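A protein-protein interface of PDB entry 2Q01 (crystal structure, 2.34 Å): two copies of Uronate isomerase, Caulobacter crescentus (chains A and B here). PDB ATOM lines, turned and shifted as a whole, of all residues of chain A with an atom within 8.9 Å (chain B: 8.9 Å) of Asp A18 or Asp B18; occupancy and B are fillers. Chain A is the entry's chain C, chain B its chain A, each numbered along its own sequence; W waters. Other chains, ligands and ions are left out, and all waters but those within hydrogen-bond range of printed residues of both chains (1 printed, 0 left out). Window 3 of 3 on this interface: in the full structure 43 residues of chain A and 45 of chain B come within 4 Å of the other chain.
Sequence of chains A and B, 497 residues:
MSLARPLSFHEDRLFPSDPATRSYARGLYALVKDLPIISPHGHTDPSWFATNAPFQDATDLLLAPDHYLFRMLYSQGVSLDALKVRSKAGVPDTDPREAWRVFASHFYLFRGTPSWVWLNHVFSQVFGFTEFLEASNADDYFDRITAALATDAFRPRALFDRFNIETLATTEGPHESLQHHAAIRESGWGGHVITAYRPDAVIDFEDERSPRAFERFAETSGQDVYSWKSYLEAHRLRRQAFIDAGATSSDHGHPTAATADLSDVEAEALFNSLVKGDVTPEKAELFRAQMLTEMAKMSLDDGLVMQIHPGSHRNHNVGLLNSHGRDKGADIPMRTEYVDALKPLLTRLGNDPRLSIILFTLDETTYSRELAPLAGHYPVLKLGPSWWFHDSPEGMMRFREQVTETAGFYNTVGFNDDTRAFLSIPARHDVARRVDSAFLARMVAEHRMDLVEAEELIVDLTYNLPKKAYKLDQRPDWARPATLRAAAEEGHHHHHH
Asp A18 touches its own counterpart, Asp B18. Ala A445 touches Arg B22, but with the chains exchanged Arg A22 does not touch Ala B445 (17.6 Å). Glu A446 touches Phe B15, but with the chains exchanged Phe A15 does not touch Glu B446 (15.8 Å). Glu A446 touches Pro B16, but with the chains exchanged Pro A16 does not touch Glu B446 (13.4 Å). Of the 9 pairs that touch across the chains among the printed residues, 1 has its exchanged pair printed and touching as well.
Among the printed residues, no Asp or Glu carboxylate lies within 4 Å of a Lys or Arg side-chain nitrogen of the other chain.
Pro A16 touches none of the printed residues of chain B. No residue of chain B comes within 4 Å of Pro A19. Of the printed residues of chain B, Thr A21 touches Ser B17. Of the printed residues of chain B, Ala A445 touches Ser B17 and Arg B22. Ser B17 touches four residues of chain A. Asp B18 touches just one residue of chain A: Asp A18. No residue of chain A comes within 4 Å of Ala B20. Of the printed residues of chain A, Arg B22 touches Ala A445 (2.8 Å) and Glu A446 (3.8 Å). The nearest printed residue of chain B that does not touch Thr A21 is Asp B18 (6.0 Å).
NH2 of Arg B22 lies within hydrogen-bond range of O of Phe B15 (2.9 Å). O of Pro B16 is in hydrogen-bond range of NE of Arg B22, 2.7 Å away. OD2 of Asp B18 sits at hydrogen-bond distance from OG1 of Thr B21. OD2 of Asp A18 lies within hydrogen-bond range of OG1 of Thr A21 (2.8 Å). The guanidinium group (NH1) of Arg A442 lies within salt-bridge range of the side-chain carboxylate (OE2) of Glu A446, at 3.3 Å.
Water W1 lies within hydrogen-bond range of the backbone NH of Ser B17 (2.8 Å) and the side-chain carboxylate of Glu A446 (3.1 Å).
CA of Asp B18 touches OD1 of Asp A18, 3.4 Å away. Ser B17 touches Ala A20 (OG to CB, 3.5 Å). Ser B17 touches Ala A445. Phe B15 touches Glu A446 (O to CG, 3.4 Å). Pro B16 touches Glu A446. Glu A446 touches Arg B22.
The side-chain carboxylate of Asp A18 sits at hydrogen-bond distance from the side-chain hydroxyl of Ser B17 (2.7 Å). The side-chain hydroxyl of Ser B17 sits at hydrogen-bond distance from the side-chain hydroxyl of Thr A21, at 3.5 Å. The guanidinium group of Arg B22 is in hydrogen-bond range of the backbone carbonyl oxygen of Ala A445, 2.8 Å away.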
ATOM      1  N   PHE A  15      25.399 -13.410   4.381  1.00  0.00           N
ATOM      2  CA  PHE A  15      25.441 -13.036   5.795  1.00  0.00           C
ATOM      3  C   PHE A  15      26.617 -12.090   5.995  1.00  0.00           C
ATOM      4  O   PHE A  15      27.624 -12.230   5.293  1.00  0.00           O
ATOM      5  CB  PHE A  15      25.601 -14.267   6.696  1.00  0.00           C
ATOM      6  CG  PHE A  15      24.488 -15.265   6.577  1.00  0.00           C
ATOM      7  CD1 PHE A  15      23.170 -14.861   6.381  1.00  0.00           C
ATOM      8  CD2 PHE A  15      24.757 -16.615   6.690  1.00  0.00           C
ATOM      9  CE1 PHE A  15      22.153 -15.799   6.277  1.00  0.00           C
ATOM     10  CE2 PHE A  15      23.750 -17.563   6.582  1.00  0.00           C
ATOM     11  CZ  PHE A  15      22.449 -17.154   6.375  1.00  0.00           C
ATOM     12  N   PRO A  16      26.506 -11.128   6.944  1.00  0.00           N
ATOM     13  CA  PRO A  16      27.602 -10.183   7.194  1.00  0.00           C
ATOM     14  C   PRO A  16      28.847 -10.888   7.719  1.00  0.00           C
ATOM     15  O   PRO A  16      28.741 -11.959   8.312  1.00  0.00           O
ATOM     16  CB  PRO A  16      27.031  -9.261   8.273  1.00  0.00           C
ATOM     17  CG  PRO A  16      25.566  -9.440   8.195  1.00  0.00           C
ATOM     18  CD  PRO A  16      25.372 -10.864   7.842  1.00  0.00           C
ATOM     19  N   SER A  17      30.015 -10.298   7.483  1.00  0.00           N
ATOM     20  CA  SER A  17      31.280 -10.928   7.850  1.00  0.00           C
ATOM     21  C   SER A  17      31.471 -11.000   9.360  1.00  0.00           C
ATOM     22  O   SER A  17      32.045 -11.963   9.866  1.00  0.00           O
ATOM     23  CB  SER A  17      32.446 -10.189   7.210  1.00  0.00           C
ATOM     24  OG  SER A  17      33.678 -10.820   7.514  1.00  0.00           O
ATOM     25  N   ASP A  18      30.983  -9.977  10.059  1.00  0.00           N
ATOM     26  CA  ASP A  18      31.009  -9.920  11.509  1.00  0.00           C
ATOM     27  C   ASP A  18      30.456 -11.213  12.077  1.00  0.00           C
ATOM     28  O   ASP A  18      29.290 -11.536  11.834  1.00  0.00           O
ATOM     29  CB  ASP A  18      30.175  -8.747  12.009  1.00  0.00           C
ATOM     30  CG  ASP A  18      30.344  -8.516  13.489  1.00  0.00           C
ATOM     31  OD1 ASP A  18      31.387  -7.949  13.880  1.00  0.00           O
ATOM     32  OD2 ASP A  18      29.441  -8.913  14.256  1.00  0.00           O
ATOM     33  N   PRO A  19      31.303 -11.968  12.810  1.00  0.00           N
ATOM     34  CA  PRO A  19      30.980 -13.334  13.221  1.00  0.00           C
ATOM     35  C   PRO A  19      29.820 -13.398  14.214  1.00  0.00           C
ATOM     36  O   PRO A  19      28.988 -14.311  14.122  1.00  0.00           O
ATOM     37  CB  PRO A  19      32.291 -13.836  13.838  1.00  0.00           C
ATOM     38  CG  PRO A  19      33.347 -12.874  13.345  1.00  0.00           C
ATOM     39  CD  PRO A  19      32.643 -11.572  13.277  1.00  0.00           C
ATOM     40  N   ALA A  20      29.763 -12.426  15.127  1.00  0.00           N
ATOM     41  CA  ALA A  20      28.631 -12.263  16.042  1.00  0.00           C
ATOM     42  C   ALA A  20      27.304 -12.130  15.285  1.00  0.00           C
ATOM     43  O   ALA A  20      26.354 -12.841  15.585  1.00  0.00           O
ATOM     44  CB  ALA A  20      28.853 -11.061  16.946  1.00  0.00           C
ATOM     45  N   THR A  21      27.269 -11.237  14.293  1.00  0.00           N
ATOM     46  CA  THR A  21      26.097 -11.024  13.432  1.00  0.00           C
ATOM     47  C   THR A  21      25.811 -12.224  12.510  1.00  0.00           C
ATOM     48  O   THR A  21      24.653 -12.601  12.307  1.00  0.00           O
ATOM     49  CB  THR A  21      26.253  -9.746  12.574  1.00  0.00           C
ATOM     50  OG1 THR A  21      26.747  -8.674  13.382  1.00  0.00           O
ATOM     51  CG2 THR A  21      24.926  -9.330  11.966  1.00  0.00           C
ATOM     52  N   ARG A  22      26.869 -12.823  11.967  1.00  0.00           N
ATOM     53  CA  ARG A  22      26.734 -13.985  11.084  1.00  0.00           C
ATOM     54  C   ARG A  22      26.146 -15.206  11.797  1.00  0.00           C
ATOM     55  O   ARG A  22      25.344 -15.946  11.214  1.00  0.00           O
ATOM     56  CB  ARG A  22      28.082 -14.334  10.456  1.00  0.00           C
ATOM     57  CG  ARG A  22      28.072 -15.580   9.599  1.00  0.00           C
ATOM     58  CD  ARG A  22      29.304 -15.685   8.748  1.00  0.00           C
ATOM     59  NE  ARG A  22      29.321 -14.686   7.683  1.00  0.00           N
ATOM     60  CZ  ARG A  22      30.093 -14.770   6.607  1.00  0.00           C
ATOM     61  NH1 ARG A  22      30.901 -15.810   6.462  1.00  0.00           N
ATOM     62  NH2 ARG A  22      30.062 -13.822   5.678  1.00  0.00           N
ATOM     63  N   SER A  23      26.547 -15.406  13.053  1.00  0.00           N
ATOM     64  CA  SER A  23      26.018 -16.487  13.880  1.00  0.00           C
ATOM     65  C   SER A  23      24.523 -16.326  14.172  1.00  0.00           C
ATOM     66  O   SER A  23      23.781 -17.312  14.118  1.00  0.00           O
ATOM     67  CB  SER A  23      26.812 -16.618  15.181  1.00  0.00           C
ATOM     68  OG  SER A  23      26.062 -17.292  16.180  1.00  0.00           O
ATOM     69  N   TYR A  24      24.088 -15.100  14.478  1.00  0.00           N
ATOM     70  CA  TYR A  24      22.650 -14.815  14.633  1.00  0.00           C
ATOM     71  C   TYR A  24      21.882 -15.035  13.325  1.00  0.00           C
ATOM     72  O   TYR A  24      20.792 -15.609  13.340  1.00  0.00           O
ATOM     73  CB  TYR A  24      22.400 -13.391  15.131  1.00  0.00           C
ATOM     74  CG  TYR A  24      22.705 -13.147  16.591  1.00  0.00           C
ATOM     75  CD1 TYR A  24      23.537 -12.096  16.974  1.00  0.00           C
ATOM     76  CD2 TYR A  24      22.153 -13.947  17.592  1.00  0.00           C
ATOM     77  CE1 TYR A  24      23.824 -11.854  18.306  1.00  0.00           C
ATOM     78  CE2 TYR A  24      22.432 -13.709  18.934  1.00  0.00           C
ATOM     79  CZ  TYR A  24      23.269 -12.659  19.279  1.00  0.00           C
ATOM     80  OH  TYR A  24      23.559 -12.409  20.598  1.00  0.00           O
ATOM     81  N   ALA A  25      22.468 -14.589  12.208  1.00  0.00           N
ATOM     82  CA  ALA A  25      21.863 -14.694  10.874  1.00  0.00           C
ATOM     83  C   ALA A  25      21.627 -16.131  10.449  1.00  0.00           C
ATOM     84  O   ALA A  25      20.521 -16.485  10.030  1.00  0.00           O
ATOM     85  CB  ALA A  25      22.726 -13.978   9.839  1.00  0.00           C
ATOM     86  N   ARG A  26      22.669 -16.949  10.574  1.00  0.00           N
ATOM     87  CA  ARG A  26      22.627 -18.368  10.231  1.00  0.00           C
ATOM     88  C   ARG A  26      21.547 -19.131  11.000  1.00  0.00           C
ATOM     89  O   ARG A  26      20.903 -20.023  10.442  1.00  0.00           O
ATOM     90  CB  ARG A  26      23.994 -19.003  10.471  1.00  0.00           C
ATOM     91  CG  ARG A  26      24.215 -20.319   9.739  1.00  0.00           C
ATOM     92  CD  ARG A  26      25.436 -21.064  10.263  1.00  0.00           C
ATOM     93  NE  ARG A  26      26.693 -20.367   9.991  1.00  0.00           N
ATOM     94  CZ  ARG A  26      27.444 -19.774  10.913  1.00  0.00           C
ATOM     95  NH1 ARG A  26      28.573 -19.173  10.555  1.00  0.00           N
ATOM     96  NH2 ARG A  26      27.074 -19.780  12.190  1.00  0.00           N
ATOM     97  N   ALA A 438      20.060 -11.512   7.646  1.00  0.00           N
ATOM     98  CA  ALA A 438      21.199 -10.614   7.859  1.00  0.00           C
ATOM     99  C   ALA A 438      20.783  -9.284   8.471  1.00  0.00           C
ATOM    100  O   ALA A 438      21.473  -8.761   9.349  1.00  0.00           O
ATOM    101  CB  ALA A 438      21.944 -10.381   6.550  1.00  0.00           C
ATOM    102  N   ALA A 441      19.493 -10.036  12.096  1.00  0.00           N
ATOM    103  CA  ALA A 441      20.659 -10.356  12.923  1.00  0.00           C
ATOM    104  C   ALA A 441      21.371  -9.103  13.401  1.00  0.00           C
ATOM    105  O   ALA A 441      21.759  -9.013  14.565  1.00  0.00           O
ATOM    106  CB  ALA A 441      21.612 -11.203  12.156  1.00  0.00           C
ATOM    107  N   ARG A 442      21.522  -8.136  12.497  1.00  0.00           N
ATOM    108  CA  ARG A 442      22.171  -6.868  12.811  1.00  0.00           C
ATOM    109  C   ARG A 442      21.402  -6.075  13.858  1.00  0.00           C
ATOM    110  O   ARG A 442      22.001  -5.333  14.632  1.00  0.00           O
ATOM    111  CB  ARG A 442      22.363  -6.043  11.546  1.00  0.00           C
ATOM    112  CG  ARG A 442      23.572  -5.131  11.580  1.00  0.00           C
ATOM    113  CD  ARG A 442      23.174  -3.681  11.709  1.00  0.00           C
ATOM    114  NE  ARG A 442      22.581  -3.176  10.474  1.00  0.00           N
ATOM    115  CZ  ARG A 442      22.227  -1.912  10.271  1.00  0.00           C
ATOM    116  NH1 ARG A 442      22.404  -1.000  11.221  1.00  0.00           N
ATOM    117  NH2 ARG A 442      21.694  -1.556   9.111  1.00  0.00           N
ATOM    118  N   ALA A 445      22.271  -8.013  17.127  1.00  0.00           N
ATOM    119  CA  ALA A 445      23.663  -7.718  17.461  1.00  0.00           C
ATOM    120  C   ALA A 445      23.882  -6.313  18.020  1.00  0.00           C
ATOM    121  O   ALA A 445      24.773  -6.101  18.848  1.00  0.00           O
ATOM    122  CB  ALA A 445      24.547  -7.950  16.254  1.00  0.00           C
ATOM    123  N   GLU A 446      23.059  -5.365  17.571  1.00  0.00           N
ATOM    124  CA  GLU A 446      23.120  -3.981  18.038  1.00  0.00           C
ATOM    125  C   GLU A 446      22.127  -3.720  19.162  1.00  0.00           C
ATOM    126  O   GLU A 446      21.995  -2.583  19.631  1.00  0.00           O
ATOM    127  CB  GLU A 446      22.868  -3.018  16.884  1.00  0.00           C
ATOM    128  CG  GLU A 446      24.005  -2.960  15.877  1.00  0.00           C
ATOM    129  CD  GLU A 446      23.785  -1.911  14.802  1.00  0.00           C
ATOM    130  OE1 GLU A 446      24.789  -1.391  14.267  1.00  0.00           O
ATOM    131  OE2 GLU A 446      22.611  -1.605  14.493  1.00  0.00           O
ATOM    132  N   PHE B  15      25.435   0.575  19.428  1.00  0.00           N
ATOM    133  CA  PHE B  15      26.819   0.549  18.979  1.00  0.00           C
ATOM    134  C   PHE B  15      26.934  -0.590  17.972  1.00  0.00           C
ATOM    135  O   PHE B  15      26.169  -1.560  18.062  1.00  0.00           O
ATOM    136  CB  PHE B  15      27.794   0.340  20.150  1.00  0.00           C
ATOM    137  CG  PHE B  15      27.667   1.358  21.253  1.00  0.00           C
ATOM    138  CD1 PHE B  15      27.250   2.668  20.995  1.00  0.00           C
ATOM    139  CD2 PHE B  15      27.995   1.008  22.557  1.00  0.00           C
ATOM    140  CE1 PHE B  15      27.139   3.599  22.026  1.00  0.00           C
ATOM    141  CE2 PHE B  15      27.890   1.931  23.593  1.00  0.00           C
ATOM    142  CZ  PHE B  15      27.457   3.225  23.331  1.00  0.00           C
ATOM    143  N   PRO B  16      27.863  -0.476  16.997  1.00  0.00           N
ATOM    144  CA  PRO B  16      28.062  -1.564  16.032  1.00  0.00           C
ATOM    145  C   PRO B  16      28.557  -2.842  16.702  1.00  0.00           C
ATOM    146  O   PRO B  16      29.228  -2.780  17.732  1.00  0.00           O
ATOM    147  CB  PRO B  16      29.149  -1.020  15.101  1.00  0.00           C
ATOM    148  CG  PRO B  16      29.115   0.447  15.287  1.00  0.00           C
ATOM    149  CD  PRO B  16      28.766   0.653  16.720  1.00  0.00           C
ATOM    150  N   SER B  17      28.214  -3.981  16.109  1.00  0.00           N
ATOM    151  CA  SER B  17      28.612  -5.295  16.607  1.00  0.00           C
ATOM    152  C   SER B  17      30.118  -5.531  16.566  1.00  0.00           C
ATOM    153  O   SER B  17      30.645  -6.272  17.397  1.00  0.00           O
ATOM    154  CB  SER B  17      27.916  -6.392  15.814  1.00  0.00           C
ATOM    155  OG  SER B  17      28.241  -7.671  16.331  1.00  0.00           O
ATOM    156  N   ASP B  18      30.790  -4.904  15.598  1.00  0.00           N
ATOM    157  CA  ASP B  18      32.234  -5.015  15.430  1.00  0.00           C
ATOM    158  C   ASP B  18      32.959  -4.571  16.688  1.00  0.00           C
ATOM    159  O   ASP B  18      32.933  -3.391  17.021  1.00  0.00           O
ATOM    160  CB  ASP B  18      32.706  -4.191  14.235  1.00  0.00           C
ATOM    161  CG  ASP B  18      34.192  -4.320  14.001  1.00  0.00           C
ATOM    162  OD1 ASP B  18      34.624  -5.408  13.559  1.00  0.00           O
ATOM    163  OD2 ASP B  18      34.921  -3.340  14.275  1.00  0.00           O
ATOM    164  N   PRO B  19      33.617  -5.527  17.377  1.00  0.00           N
ATOM    165  CA  PRO B  19      34.166  -5.411  18.734  1.00  0.00           C
ATOM    166  C   PRO B  19      35.148  -4.259  18.952  1.00  0.00           C
ATOM    167  O   PRO B  19      35.147  -3.653  20.028  1.00  0.00           O
ATOM    168  CB  PRO B  19      34.869  -6.758  18.934  1.00  0.00           C
ATOM    169  CG  PRO B  19      34.123  -7.691  18.041  1.00  0.00           C
ATOM    170  CD  PRO B  19      33.879  -6.867  16.818  1.00  0.00           C
ATOM    171  N   ALA B  20      35.971  -3.969  17.947  1.00  0.00           N
ATOM    172  CA  ALA B  20      36.920  -2.860  18.018  1.00  0.00           C
ATOM    173  C   ALA B  20      36.198  -1.523  17.938  1.00  0.00           C
ATOM    174  O   ALA B  20      36.418  -0.650  18.776  1.00  0.00           O
ATOM    175  CB  ALA B  20      37.966  -2.972  16.917  1.00  0.00           C
ATOM    176  N   THR B  21      35.327  -1.386  16.936  1.00  0.00           N
ATOM    177  CA  THR B  21      34.487  -0.197  16.752  1.00  0.00           C
ATOM    178  C   THR B  21      33.607   0.049  17.985  1.00  0.00           C
ATOM    179  O   THR B  21      33.506   1.184  18.455  1.00  0.00           O
ATOM    180  CB  THR B  21      33.618  -0.302  15.461  1.00  0.00           C
ATOM    181  OG1 THR B  21      34.463  -0.525  14.325  1.00  0.00           O
ATOM    182  CG2 THR B  21      32.834   0.963  15.221  1.00  0.00           C
ATOM    183  N   ARG B  22      33.010  -1.024  18.514  1.00  0.00           N
ATOM    184  CA  ARG B  22      32.186  -0.968  19.731  1.00  0.00           C
ATOM    185  C   ARG B  22      32.938  -0.427  20.942  1.00  0.00           C
ATOM    186  O   ARG B  22      32.399   0.380  21.702  1.00  0.00           O
ATOM    187  CB  ARG B  22      31.605  -2.346  20.058  1.00  0.00           C
ATOM    188  CG  ARG B  22      30.635  -2.347  21.239  1.00  0.00           C
ATOM    189  CD  ARG B  22      29.792  -3.606  21.262  1.00  0.00           C
ATOM    190  NE  ARG B  22      28.695  -3.533  20.306  1.00  0.00           N
ATOM    191  CZ  ARG B  22      27.593  -4.274  20.359  1.00  0.00           C
ATOM    192  NH1 ARG B  22      27.425  -5.164  21.326  1.00  0.00           N
ATOM    193  NH2 ARG B  22      26.655  -4.118  19.438  1.00  0.00           N
ATOM    194  N   SER B  23      34.180  -0.869  21.108  1.00  0.00           N
ATOM    195  CA  SER B  23      35.018  -0.427  22.213  1.00  0.00           C
ATOM    196  C   SER B  23      35.311   1.073  22.155  1.00  0.00           C
ATOM    197  O   SER B  23      35.344   1.744  23.193  1.00  0.00           O
ATOM    198  CB  SER B  23      36.317  -1.225  22.241  1.00  0.00           C
ATOM    199  OG  SER B  23      37.116  -0.823  23.337  1.00  0.00           O
ATOM    200  N   TYR B  24      35.523   1.585  20.942  1.00  0.00           N
ATOM    201  CA  TYR B  24      35.672   3.022  20.714  1.00  0.00           C
ATOM    202  C   TYR B  24      34.374   3.770  21.027  1.00  0.00           C
ATOM    203  O   TYR B  24      34.393   4.781  21.725  1.00  0.00           O
ATOM    204  CB  TYR B  24      36.075   3.304  19.269  1.00  0.00           C
ATOM    205  CG  TYR B  24      37.513   3.020  18.936  1.00  0.00           C
ATOM    206  CD1 TYR B  24      37.844   2.163  17.887  1.00  0.00           C
ATOM    207  CD2 TYR B  24      38.544   3.621  19.646  1.00  0.00           C
ATOM    208  CE1 TYR B  24      39.166   1.901  17.565  1.00  0.00           C
ATOM    209  CE2 TYR B  24      39.869   3.374  19.328  1.00  0.00           C
ATOM    210  CZ  TYR B  24      40.173   2.513  18.290  1.00  0.00           C
ATOM    211  OH  TYR B  24      41.488   2.266  17.979  1.00  0.00           O
ATOM    212  N   ALA B  25      33.257   3.253  20.515  1.00  0.00           N
ATOM    213  CA  ALA B  25      31.937   3.831  20.756  1.00  0.00           C
ATOM    214  C   ALA B  25      31.636   3.962  22.243  1.00  0.00           C
ATOM    215  O   ALA B  25      31.185   5.017  22.695  1.00  0.00           O
ATOM    216  CB  ALA B  25      30.864   3.002  20.067  1.00  0.00           C
ATOM    217  N   ARG B  26      31.926   2.897  22.990  1.00  0.00           N
ATOM    218  CA  ARG B  26      31.639   2.807  24.422  1.00  0.00           C
ATOM    219  C   ARG B  26      32.432   3.851  25.217  1.00  0.00           C
ATOM    220  O   ARG B  26      31.924   4.424  26.186  1.00  0.00           O
ATOM    221  CB  ARG B  26      31.952   1.394  24.922  1.00  0.00           C
ATOM    222  CG  ARG B  26      31.051   0.920  26.040  1.00  0.00           C
ATOM    223  CD  ARG B  26      31.605  -0.330  26.711  1.00  0.00           C
ATOM    224  NE  ARG B  26      31.227  -1.570  26.033  1.00  0.00           N
ATOM    225  CZ  ARG B  26      32.068  -2.384  25.391  1.00  0.00           C
ATOM    226  NH1 ARG B  26      31.602  -3.490  24.824  1.00  0.00           N
ATOM    227  NH2 ARG B  26      33.365  -2.105  25.317  1.00  0.00           N
ATOM    228  N   ALA B 438      28.767   5.936  17.815  1.00  0.00           N
ATOM    229  CA  ALA B 438      28.889   4.871  16.821  1.00  0.00           C
ATOM    230  C   ALA B 438      29.530   5.340  15.526  1.00  0.00           C
ATOM    231  O   ALA B 438      30.414   4.668  14.990  1.00  0.00           O
ATOM    232  CB  ALA B 438      27.516   4.249  16.534  1.00  0.00           C
ATOM    233  N   ALA B 441      33.197   6.418  16.157  1.00  0.00           N
ATOM    234  CA  ALA B 441      33.942   5.165  16.360  1.00  0.00           C
ATOM    235  C   ALA B 441      34.321   4.466  15.057  1.00  0.00           C
ATOM    236  O   ALA B 441      35.429   3.948  14.932  1.00  0.00           O
ATOM    237  CB  ALA B 441      33.153   4.220  17.219  1.00  0.00           C
ATOM    238  N   ARG B 442      33.395   4.453  14.100  1.00  0.00           N
ATOM    239  CA  ARG B 442      33.627   3.863  12.785  1.00  0.00           C
ATOM    240  C   ARG B 442      34.663   4.647  11.979  1.00  0.00           C
ATOM    241  O   ARG B 442      35.355   4.071  11.144  1.00  0.00           O
ATOM    242  CB  ARG B 442      32.325   3.790  11.996  1.00  0.00           C
ATOM    243  CG  ARG B 442      32.100   2.454  11.303  1.00  0.00           C
ATOM    244  CD  ARG B 442      31.907   2.591   9.799  1.00  0.00           C
ATOM    245  NE  ARG B 442      30.960   3.637   9.419  1.00  0.00           N
ATOM    246  CZ  ARG B 442      30.878   4.159   8.198  1.00  0.00           C
ATOM    247  NH1 ARG B 442      31.688   3.739   7.232  1.00  0.00           N
ATOM    248  NH2 ARG B 442      29.991   5.111   7.944  1.00  0.00           N
ATOM    249  N   ALA B 445      38.091   3.644  13.843  1.00  0.00           N
ATOM    250  CA  ALA B 445      38.390   2.262  13.461  1.00  0.00           C
ATOM    251  C   ALA B 445      38.861   2.113  12.010  1.00  0.00           C
ATOM    252  O   ALA B 445      39.618   1.193  11.699  1.00  0.00           O
ATOM    253  CB  ALA B 445      37.183   1.376  13.718  1.00  0.00           C
ATOM    254  N   GLU B 446      38.416   3.014  11.132  1.00  0.00           N
ATOM    255  CA  GLU B 446      38.859   3.021   9.733  1.00  0.00           C
ATOM    256  C   GLU B 446      39.971   4.039   9.514  1.00  0.00           C
ATOM    257  O   GLU B 446      40.380   4.278   8.375  1.00  0.00           O
ATOM    258  CB  GLU B 446      37.696   3.311   8.789  1.00  0.00           C
ATOM    259  CG  GLU B 446      36.627   2.230   8.762  1.00  0.00           C
ATOM    260  CD  GLU B 446      35.545   2.501   7.732  1.00  0.00           C
ATOM    261  OE1 GLU B 446      34.516   1.794   7.762  1.00  0.00           O
ATOM    262  OE2 GLU B 446      35.720   3.413   6.892  1.00  0.00           O
HETATM  263  O   HOH W   1      26.754  -3.685  13.699  1.00  0.00           O
